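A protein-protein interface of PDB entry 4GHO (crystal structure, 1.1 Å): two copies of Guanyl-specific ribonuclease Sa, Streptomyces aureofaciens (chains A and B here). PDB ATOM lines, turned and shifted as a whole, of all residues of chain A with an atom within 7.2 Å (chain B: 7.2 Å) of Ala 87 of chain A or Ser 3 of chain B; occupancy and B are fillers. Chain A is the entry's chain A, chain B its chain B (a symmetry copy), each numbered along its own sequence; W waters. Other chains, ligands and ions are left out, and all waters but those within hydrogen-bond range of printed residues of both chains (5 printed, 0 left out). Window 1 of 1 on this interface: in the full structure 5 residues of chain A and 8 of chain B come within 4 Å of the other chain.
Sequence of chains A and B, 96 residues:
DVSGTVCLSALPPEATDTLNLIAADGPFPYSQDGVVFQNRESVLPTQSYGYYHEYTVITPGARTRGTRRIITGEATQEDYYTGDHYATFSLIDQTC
Of the printed residues of chain B, Glu 41 of chain A touches Ser 3 (3.7 Å) and Gly 4 (3.5 Å).
Of chain B, only Ser 3 (3.4 Å) and Thr 88 (3.8 Å) come within 4 Å of Ala 87 of chain A.
Asp 1 of chain B touches none of the printed residues of chain A.
Ser 3 of chain B touches two residues of chain A.
Printed residues of chain A within 4 Å of Gly 4 of chain B: Glu 41.
Of the printed residues of chain A, Thr 88 of chain B touches Ala 87.
Ser 90 of chain B touches none of the printed residues of chain A.
OD1 of Asp 84 of chain B sits at hydrogen-bond distance from OG1 of Thr 88 of chain B, 2.7 Å away.
The backbone NH of Ser 3 of chain B is in hydrogen-bond range of the backbone carbonyl oxygen of Phe 89 of chain B, at 2.8 Å.
The backbone carbonyl oxygen (O) of Gly 4 of chain B is in hydrogen-bond range of the backbone NH (N) of Leu 91 of chain B.
The backbone NH (N) of Ala 87 of chain A lies within hydrogen-bond range of the side-chain carboxylate (OD2) of Asp 84 of chain A (3.2 Å).
Water W5 lies within hydrogen-bond range of OE1 of Glu 41 of chain A and O of Ser 3 of chain B.
Water W2 lies within hydrogen-bond range of O of Ser 3 of chain B (2.6 Å) and O of Tyr 86 of chain A (2.7 Å).
Water W1 bridges OE2 of Glu 41 of chain A (2.6 Å) and N of Thr 5 of chain B (3.0 Å).
Water W3 bridges the side-chain hydroxyl (OG) of Ser 90 of chain B (2.7 Å) and a ring nitrogen (ND1) of His 85 of chain A (2.9 Å).
Water W4 lies within hydrogen-bond range of OG1 of Thr 88 of chain B (2.8 Å), O of Asp 84 of chain A (2.8 Å) and OG of Ser 3 of chain B (3.4 Å).
Ala 87 of chain A touches Ser 3 of chain B, but with the chains exchanged Ser 3 of chain A does not touch Ala 87 of chain B (12.7 Å).
Ala 87 of chain A touches Thr 88 of chain B, but with the chains exchanged Thr 88 of chain A does not touch Ala 87 of chain B (8.5 Å).
Of the 4 pairs that touch across the chains among the printed residues, none has its exchanged pair printed and touching as well.
Among the printed residues, pairs that only touch across the chains: Ala 87 of chain A with Ser 3 of chain B (3.4 Å), Glu 41 of chain A with Gly 4 of chain B (3.5 Å), Glu 41 of chain A with Ser 3 of chain B (3.7 Å) and Ala 87 of chain A with Thr 88 of chain B (3.8 Å).
Of the 12 printed residues of chain B, 3 touch a printed residue of chain A.
Of the 14 printed residues of chain A, 2 touch a printed residue of chain B.
Among the printed residues, 4 pairs touch across the chains.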
ATOM      1  N   ASP A   1       2.742 -12.548 -27.662  1.00  0.00           N
ATOM      2  CA  ASP A   1       1.339 -12.317 -27.297  1.00  0.00           C
ATOM      3  C   ASP A   1       0.738 -13.620 -26.750  1.00  0.00           C
ATOM      4  O   ASP A   1       1.223 -14.677 -27.057  1.00  0.00           O
ATOM      5  CB  ASP A   1       0.510 -11.875 -28.530  1.00  0.00           C
ATOM      6  CG  ASP A   1       0.894 -10.507 -29.019  1.00  0.00           C
ATOM      7  OD1 ASP A   1       1.928  -9.975 -28.552  1.00  0.00           O
ATOM      8  OD2 ASP A   1       0.157  -9.937 -29.795  1.00  0.00           O
ATOM      9  N   SER A   3      -2.384 -16.173 -26.681  1.00  0.00           N
ATOM     10  CA  SER A   3      -3.361 -16.563 -27.611  1.00  0.00           C
ATOM     11  C   SER A   3      -4.788 -16.359 -27.255  1.00  0.00           C
ATOM     12  O   SER A   3      -5.667 -16.020 -28.131  1.00  0.00           O
ATOM     13  CB  SER A   3      -3.018 -17.934 -28.205  1.00  0.00           C
ATOM     14  OG  SER A   3      -1.789 -17.760 -28.916  1.00  0.00           O
ATOM     15  N   PHE A  37      11.510 -19.117 -15.730  1.00  0.00           N
ATOM     16  CA  PHE A  37      11.304 -18.998 -17.178  1.00  0.00           C
ATOM     17  C   PHE A  37      11.678 -17.577 -17.561  1.00  0.00           C
ATOM     18  O   PHE A  37      11.110 -16.626 -17.074  1.00  0.00           O
ATOM     19  CB  PHE A  37       9.853 -19.269 -17.501  1.00  0.00           C
ATOM     20  CG  PHE A  37       9.545 -19.122 -18.949  1.00  0.00           C
ATOM     21  CD1 PHE A  37       8.790 -18.057 -19.434  1.00  0.00           C
ATOM     22  CD2 PHE A  37      10.020 -20.041 -19.856  1.00  0.00           C
ATOM     23  CE1 PHE A  37       8.517 -17.923 -20.752  1.00  0.00           C
ATOM     24  CE2 PHE A  37       9.740 -19.885 -21.228  1.00  0.00           C
ATOM     25  CZ  PHE A  37       9.000 -18.806 -21.648  1.00  0.00           C
ATOM     26  N   GLU A  41      12.103 -14.655 -25.513  1.00  0.00           N
ATOM     27  CA  GLU A  41      11.520 -14.319 -26.787  1.00  0.00           C
ATOM     28  C   GLU A  41      10.434 -13.305 -26.666  1.00  0.00           C
ATOM     29  O   GLU A  41       9.846 -12.912 -27.667  1.00  0.00           O
ATOM     30  CB  GLU A  41      11.075 -15.579 -27.521  1.00  0.00           C
ATOM     31  CG  GLU A  41      12.188 -16.498 -27.908  1.00  0.00           C
ATOM     32  CD  GLU A  41      12.872 -17.262 -26.819  1.00  0.00           C
ATOM     33  OE1 GLU A  41      12.181 -17.578 -25.743  1.00  0.00           O
ATOM     34  OE2 GLU A  41      14.065 -17.418 -26.990  1.00  0.00           O
ATOM     35  N   VAL A  43       7.376 -13.495 -25.626  1.00  0.00           N
ATOM     36  CA  VAL A  43       6.024 -13.916 -25.983  1.00  0.00           C
ATOM     37  C   VAL A  43       5.019 -13.503 -24.911  1.00  0.00           C
ATOM     38  O   VAL A  43       3.902 -13.104 -25.196  1.00  0.00           O
ATOM     39  CB  VAL A  43       5.988 -15.402 -26.290  1.00  0.00           C
ATOM     40  CG1 VAL A  43       4.576 -15.827 -26.676  1.00  0.00           C
ATOM     41  CG2 VAL A  43       6.916 -15.739 -27.437  1.00  0.00           C
ATOM     42  N   THR A  67       6.568 -31.549 -24.540  1.00  0.00           N
ATOM     43  CA  THR A  67       6.350 -30.190 -25.041  1.00  0.00           C
ATOM     44  C   THR A  67       5.380 -29.395 -24.251  1.00  0.00           C
ATOM     45  O   THR A  67       5.163 -28.233 -24.614  1.00  0.00           O
ATOM     46  CB  THR A  67       5.972 -30.235 -26.501  1.00  0.00           C
ATOM     47  OG1 THR A  67       4.668 -30.743 -26.643  1.00  0.00           O
ATOM     48  CG2 THR A  67       7.007 -30.968 -27.349  1.00  0.00           C
ATOM     49  N   THR A  82       1.315 -23.962 -22.406  1.00  0.00           N
ATOM     50  CA  THR A  82       1.834 -24.174 -23.737  1.00  0.00           C
ATOM     51  C   THR A  82       1.824 -25.645 -24.000  1.00  0.00           C
ATOM     52  O   THR A  82       2.281 -26.445 -23.182  1.00  0.00           O
ATOM     53  CB  THR A  82       3.230 -23.571 -23.928  1.00  0.00           C
ATOM     54  OG1 THR A  82       3.695 -23.864 -25.257  1.00  0.00           O
ATOM     55  CG2 THR A  82       4.271 -24.048 -22.981  1.00  0.00           C
ATOM     56  N   GLY A  83       1.370 -26.039 -25.181  1.00  0.00           N
ATOM     57  CA  GLY A  83       1.461 -27.404 -25.635  1.00  0.00           C
ATOM     58  C   GLY A  83       2.456 -27.630 -26.721  1.00  0.00           C
ATOM     59  O   GLY A  83       2.587 -28.750 -27.173  1.00  0.00           O
ATOM     60  N   ASP A  84       3.175 -26.613 -27.120  1.00  0.00           N
ATOM     61  CA  ASP A  84       4.036 -26.650 -28.289  1.00  0.00           C
ATOM     62  C   ASP A  84       5.412 -26.112 -27.975  1.00  0.00           C
ATOM     63  O   ASP A  84       6.053 -25.464 -28.811  1.00  0.00           O
ATOM     64  CB  ASP A  84       3.372 -25.905 -29.428  1.00  0.00           C
ATOM     65  CG  ASP A  84       3.051 -24.479 -29.131  1.00  0.00           C
ATOM     66  OD1 ASP A  84       2.326 -23.866 -29.959  1.00  0.00           O
ATOM     67  OD2 ASP A  84       3.449 -23.934 -28.095  1.00  0.00           O
ATOM     68  N   HIS A  85       5.885 -26.415 -26.788  1.00  0.00           N
ATOM     69  CA  HIS A  85       7.243 -26.121 -26.472  1.00  0.00           C
ATOM     70  C   HIS A  85       7.540 -24.624 -26.615  1.00  0.00           C
ATOM     71  O   HIS A  85       8.497 -24.227 -27.242  1.00  0.00           O
ATOM     72  CB  HIS A  85       8.175 -26.999 -27.249  1.00  0.00           C
ATOM     73  CG  HIS A  85       9.436 -27.246 -26.555  1.00  0.00           C
ATOM     74  ND1 HIS A  85      10.445 -26.367 -26.726  1.00  0.00           N
ATOM     75  CD2 HIS A  85       9.896 -28.193 -25.768  1.00  0.00           C
ATOM     76  CE1 HIS A  85      11.547 -26.830 -26.061  1.00  0.00           C
ATOM     77  NE2 HIS A  85      11.197 -27.967 -25.496  1.00  0.00           N
ATOM     78  N   TYR A  86       6.691 -23.816 -25.999  1.00  0.00           N
ATOM     79  CA  TYR A  86       6.888 -22.404 -25.759  1.00  0.00           C
ATOM     80  C   TYR A  86       6.621 -21.530 -26.960  1.00  0.00           C
ATOM     81  O   TYR A  86       6.916 -20.353 -26.931  1.00  0.00           O
ATOM     82  CB  TYR A  86       8.264 -22.032 -25.112  1.00  0.00           C
ATOM     83  CG  TYR A  86       8.794 -22.982 -24.046  1.00  0.00           C
ATOM     84  CD1 TYR A  86       8.416 -22.864 -22.742  1.00  0.00           C
ATOM     85  CD2 TYR A  86       9.673 -23.994 -24.316  1.00  0.00           C
ATOM     86  CE1 TYR A  86       8.942 -23.647 -21.733  1.00  0.00           C
ATOM     87  CE2 TYR A  86      10.168 -24.810 -23.286  1.00  0.00           C
ATOM     88  CZ  TYR A  86       9.812 -24.617 -22.021  1.00  0.00           C
ATOM     89  OH  TYR A  86      10.337 -25.471 -21.029  1.00  0.00           O
ATOM     90  N   ALA A  87       6.063 -22.102 -28.050  1.00  0.00           N
ATOM     91  CA  ALA A  87       5.710 -21.310 -29.252  1.00  0.00           C
ATOM     92  C   ALA A  87       4.505 -20.462 -28.986  1.00  0.00           C
ATOM     93  O   ALA A  87       4.514 -19.288 -29.376  1.00  0.00           O
ATOM     94  CB  ALA A  87       5.473 -22.239 -30.457  1.00  0.00           C
ATOM     95  N   THR A  88       3.460 -21.012 -28.401  1.00  0.00           N
ATOM     96  CA  THR A  88       2.229 -20.326 -28.118  1.00  0.00           C
ATOM     97  C   THR A  88       1.774 -20.617 -26.699  1.00  0.00           C
ATOM     98  O   THR A  88       2.089 -21.667 -26.141  1.00  0.00           O
ATOM     99  CB  THR A  88       1.115 -20.658 -29.090  1.00  0.00           C
ATOM    100  OG1 THR A  88       0.686 -21.967 -28.925  1.00  0.00           O
ATOM    101  CG2 THR A  88       1.522 -20.444 -30.549  1.00  0.00           C
ATOM    102  N   PHE A  89       1.056 -19.674 -26.120  1.00  0.00           N
ATOM    103  CA  PHE A  89       0.576 -19.764 -24.786  1.00  0.00           C
ATOM    104  C   PHE A  89      -0.874 -19.351 -24.712  1.00  0.00           C
ATOM    105  O   PHE A  89      -1.273 -18.411 -25.380  1.00  0.00           O
ATOM    106  CB  PHE A  89       1.354 -18.855 -23.859  1.00  0.00           C
ATOM    107  CG  PHE A  89       2.789 -19.184 -23.714  1.00  0.00           C
ATOM    108  CD1 PHE A  89       3.719 -18.653 -24.569  1.00  0.00           C
ATOM    109  CD2 PHE A  89       3.230 -19.991 -22.686  1.00  0.00           C
ATOM    110  CE1 PHE A  89       5.060 -18.895 -24.443  1.00  0.00           C
ATOM    111  CE2 PHE A  89       4.606 -20.274 -22.552  1.00  0.00           C
ATOM    112  CZ  PHE A  89       5.481 -19.679 -23.421  1.00  0.00           C
ATOM    113  N   ASP B   1       9.339 -17.275 -37.104  1.00  0.00           N
ATOM    114  CA  ASP B   1      10.281 -16.968 -36.001  1.00  0.00           C
ATOM    115  C   ASP B   1      10.644 -18.318 -35.383  1.00  0.00           C
ATOM    116  O   ASP B   1       9.867 -19.244 -35.421  1.00  0.00           O
ATOM    117  CB  ASP B   1       9.662 -16.067 -34.912  1.00  0.00           C
ATOM    118  CG  ASP B   1       9.220 -14.734 -35.364  1.00  0.00           C
ATOM    119  OD1 ASP B   1       9.046 -13.829 -34.454  1.00  0.00           O
ATOM    120  OD2 ASP B   1       9.077 -14.563 -36.606  1.00  0.00           O
ATOM    121  N   VAL B   2      11.817 -18.402 -34.880  1.00  0.00           N
ATOM    122  CA  VAL B   2      12.242 -19.508 -34.154  1.00  0.00           C
ATOM    123  C   VAL B   2      11.656 -19.383 -32.714  1.00  0.00           C
ATOM    124  O   VAL B   2      11.620 -18.286 -32.184  1.00  0.00           O
ATOM    125  CB  VAL B   2      13.822 -19.542 -34.267  1.00  0.00           C
ATOM    126  CG1 VAL B   2      14.470 -20.583 -33.421  1.00  0.00           C
ATOM    127  CG2 VAL B   2      14.301 -19.692 -35.724  1.00  0.00           C
ATOM    128  N   SER B   3      11.124 -20.474 -32.110  1.00  0.00           N
ATOM    129  CA  SER B   3      10.419 -20.514 -30.761  1.00  0.00           C
ATOM    130  C   SER B   3      11.261 -20.344 -29.571  1.00  0.00           C
ATOM    131  O   SER B   3      10.743 -19.884 -28.499  1.00  0.00           O
ATOM    132  CB  SER B   3       9.661 -21.801 -30.528  1.00  0.00           C
ATOM    133  OG  SER B   3       8.719 -21.884 -31.511  1.00  0.00           O
ATOM    134  N   GLY B   4      12.551 -20.483 -29.770  1.00  0.00           N
ATOM    135  CA  GLY B   4      13.511 -20.362 -28.706  1.00  0.00           C
ATOM    136  C   GLY B   4      14.660 -21.264 -28.968  1.00  0.00           C
ATOM    137  O   GLY B   4      14.790 -21.850 -30.031  1.00  0.00           O
ATOM    138  N   THR B   5      15.514 -21.407 -27.995  1.00  0.00           N
ATOM    139  CA  THR B   5      16.638 -22.329 -28.008  1.00  0.00           C
ATOM    140  C   THR B   5      16.324 -23.470 -27.056  1.00  0.00           C
ATOM    141  O   THR B   5      15.779 -23.227 -25.971  1.00  0.00           O
ATOM    142  CB  THR B   5      17.905 -21.625 -27.615  1.00  0.00           C
ATOM    143  OG1 THR B   5      18.118 -20.524 -28.515  1.00  0.00           O
ATOM    144  CG2 THR B   5      19.099 -22.437 -27.571  1.00  0.00           C
ATOM    145  N   VAL B  43       9.059 -19.698 -41.821  1.00  0.00           N
ATOM    146  CA  VAL B  43       9.224 -19.760 -40.396  1.00  0.00           C
ATOM    147  C   VAL B  43      10.649 -19.453 -39.940  1.00  0.00           C
ATOM    148  O   VAL B  43      10.933 -18.769 -38.952  1.00  0.00           O
ATOM    149  CB  VAL B  43       8.716 -21.086 -39.794  1.00  0.00           C
ATOM    150  CG1 VAL B  43       8.961 -21.128 -38.268  1.00  0.00           C
ATOM    151  CG2 VAL B  43       7.217 -21.277 -40.179  1.00  0.00           C
ATOM    152  N   ASP B  84       6.988 -31.121 -34.806  1.00  0.00           N
ATOM    153  CA  ASP B  84       5.604 -30.962 -35.261  1.00  0.00           C
ATOM    154  C   ASP B  84       5.541 -30.775 -36.744  1.00  0.00           C
ATOM    155  O   ASP B  84       4.681 -30.086 -37.272  1.00  0.00           O
ATOM    156  CB  ASP B  84       4.915 -29.868 -34.484  1.00  0.00           C
ATOM    157  CG  ASP B  84       5.612 -28.539 -34.551  1.00  0.00           C
ATOM    158  OD1 ASP B  84       5.234 -27.655 -33.748  1.00  0.00           O
ATOM    159  OD2 ASP B  84       6.495 -28.355 -35.401  1.00  0.00           O
ATOM    160  N   ALA B  87       6.037 -27.071 -38.275  1.00  0.00           N
ATOM    161  CA  ALA B  87       5.239 -26.005 -37.847  1.00  0.00           C
ATOM    162  C   ALA B  87       6.009 -24.989 -37.009  1.00  0.00           C
ATOM    163  O   ALA B  87       5.816 -23.781 -37.140  1.00  0.00           O
ATOM    164  CB  ALA B  87       3.964 -26.477 -37.121  1.00  0.00           C
ATOM    165  N   THR B  88       6.777 -25.488 -36.058  1.00  0.00           N
ATOM    166  CA  THR B  88       7.571 -24.687 -35.187  1.00  0.00           C
ATOM    167  C   THR B  88       8.979 -25.273 -35.098  1.00  0.00           C
ATOM    168  O   THR B  88       9.183 -26.439 -35.338  1.00  0.00           O
ATOM    169  CB  THR B  88       6.984 -24.603 -33.799  1.00  0.00           C
ATOM    170  OG1 THR B  88       7.094 -25.818 -33.100  1.00  0.00           O
ATOM    171  CG2 THR B  88       5.527 -24.076 -33.802  1.00  0.00           C
ATOM    172  N   PHE B  89       9.917 -24.406 -34.775  1.00  0.00           N
ATOM    173  CA  PHE B  89      11.317 -24.759 -34.709  1.00  0.00           C
ATOM    174  C   PHE B  89      11.987 -24.145 -33.529  1.00  0.00           C
ATOM    175  O   PHE B  89      11.694 -23.025 -33.149  1.00  0.00           O
ATOM    176  CB  PHE B  89      12.088 -24.251 -35.934  1.00  0.00           C
ATOM    177  CG  PHE B  89      11.734 -24.902 -37.222  1.00  0.00           C
ATOM    178  CD1 PHE B  89      10.745 -24.355 -37.979  1.00  0.00           C
ATOM    179  CD2 PHE B  89      12.405 -26.031 -37.678  1.00  0.00           C
ATOM    180  CE1 PHE B  89      10.376 -24.888 -39.180  1.00  0.00           C
ATOM    181  CE2 PHE B  89      12.054 -26.618 -38.885  1.00  0.00           C
ATOM    182  CZ  PHE B  89      11.067 -26.011 -39.567  1.00  0.00           C
ATOM    183  N   SER B  90      12.944 -24.844 -32.961  1.00  0.00           N
ATOM    184  CA  SER B  90      13.822 -24.333 -31.924  1.00  0.00           C
ATOM    185  C   SER B  90      15.262 -24.506 -32.365  1.00  0.00           C
ATOM    186  O   SER B  90      15.623 -25.471 -33.005  1.00  0.00           O
ATOM    187  CB  SER B  90      13.632 -25.097 -30.627  1.00  0.00           C
ATOM    188  OG  SER B  90      12.309 -25.032 -30.137  1.00  0.00           O
ATOM    189  N   LEU B  91      16.094 -23.546 -32.043  1.00  0.00           N
ATOM    190  CA  LEU B  91      17.511 -23.674 -32.252  1.00  0.00           C
ATOM    191  C   LEU B  91      18.117 -24.616 -31.228  1.00  0.00           C
ATOM    192  O   LEU B  91      17.827 -24.484 -30.059  1.00  0.00           O
ATOM    193  CB  LEU B  91      18.195 -22.296 -32.137  1.00  0.00           C
ATOM    194  CG  LEU B  91      19.663 -22.196 -32.386  1.00  0.00           C
ATOM    195  CD1 LEU B  91      19.913 -22.400 -33.867  1.00  0.00           C
ATOM    196  CD2 LEU B  91      20.149 -20.820 -31.982  1.00  0.00           C
HETATM  197  O   HOH W   1      14.814 -19.566 -25.730  1.00  0.00           O
HETATM  198  O   HOH W   2       8.534 -18.573 -28.184  1.00  0.00           O
HETATM  199  O   HOH W   3      11.378 -23.830 -27.863  1.00  0.00           O
HETATM  200  O   HOH W   4       8.123 -25.074 -30.643  1.00  0.00           O
HETATM  201  O   HOH W   5      11.014 -19.724 -25.506  1.00  0.00           O
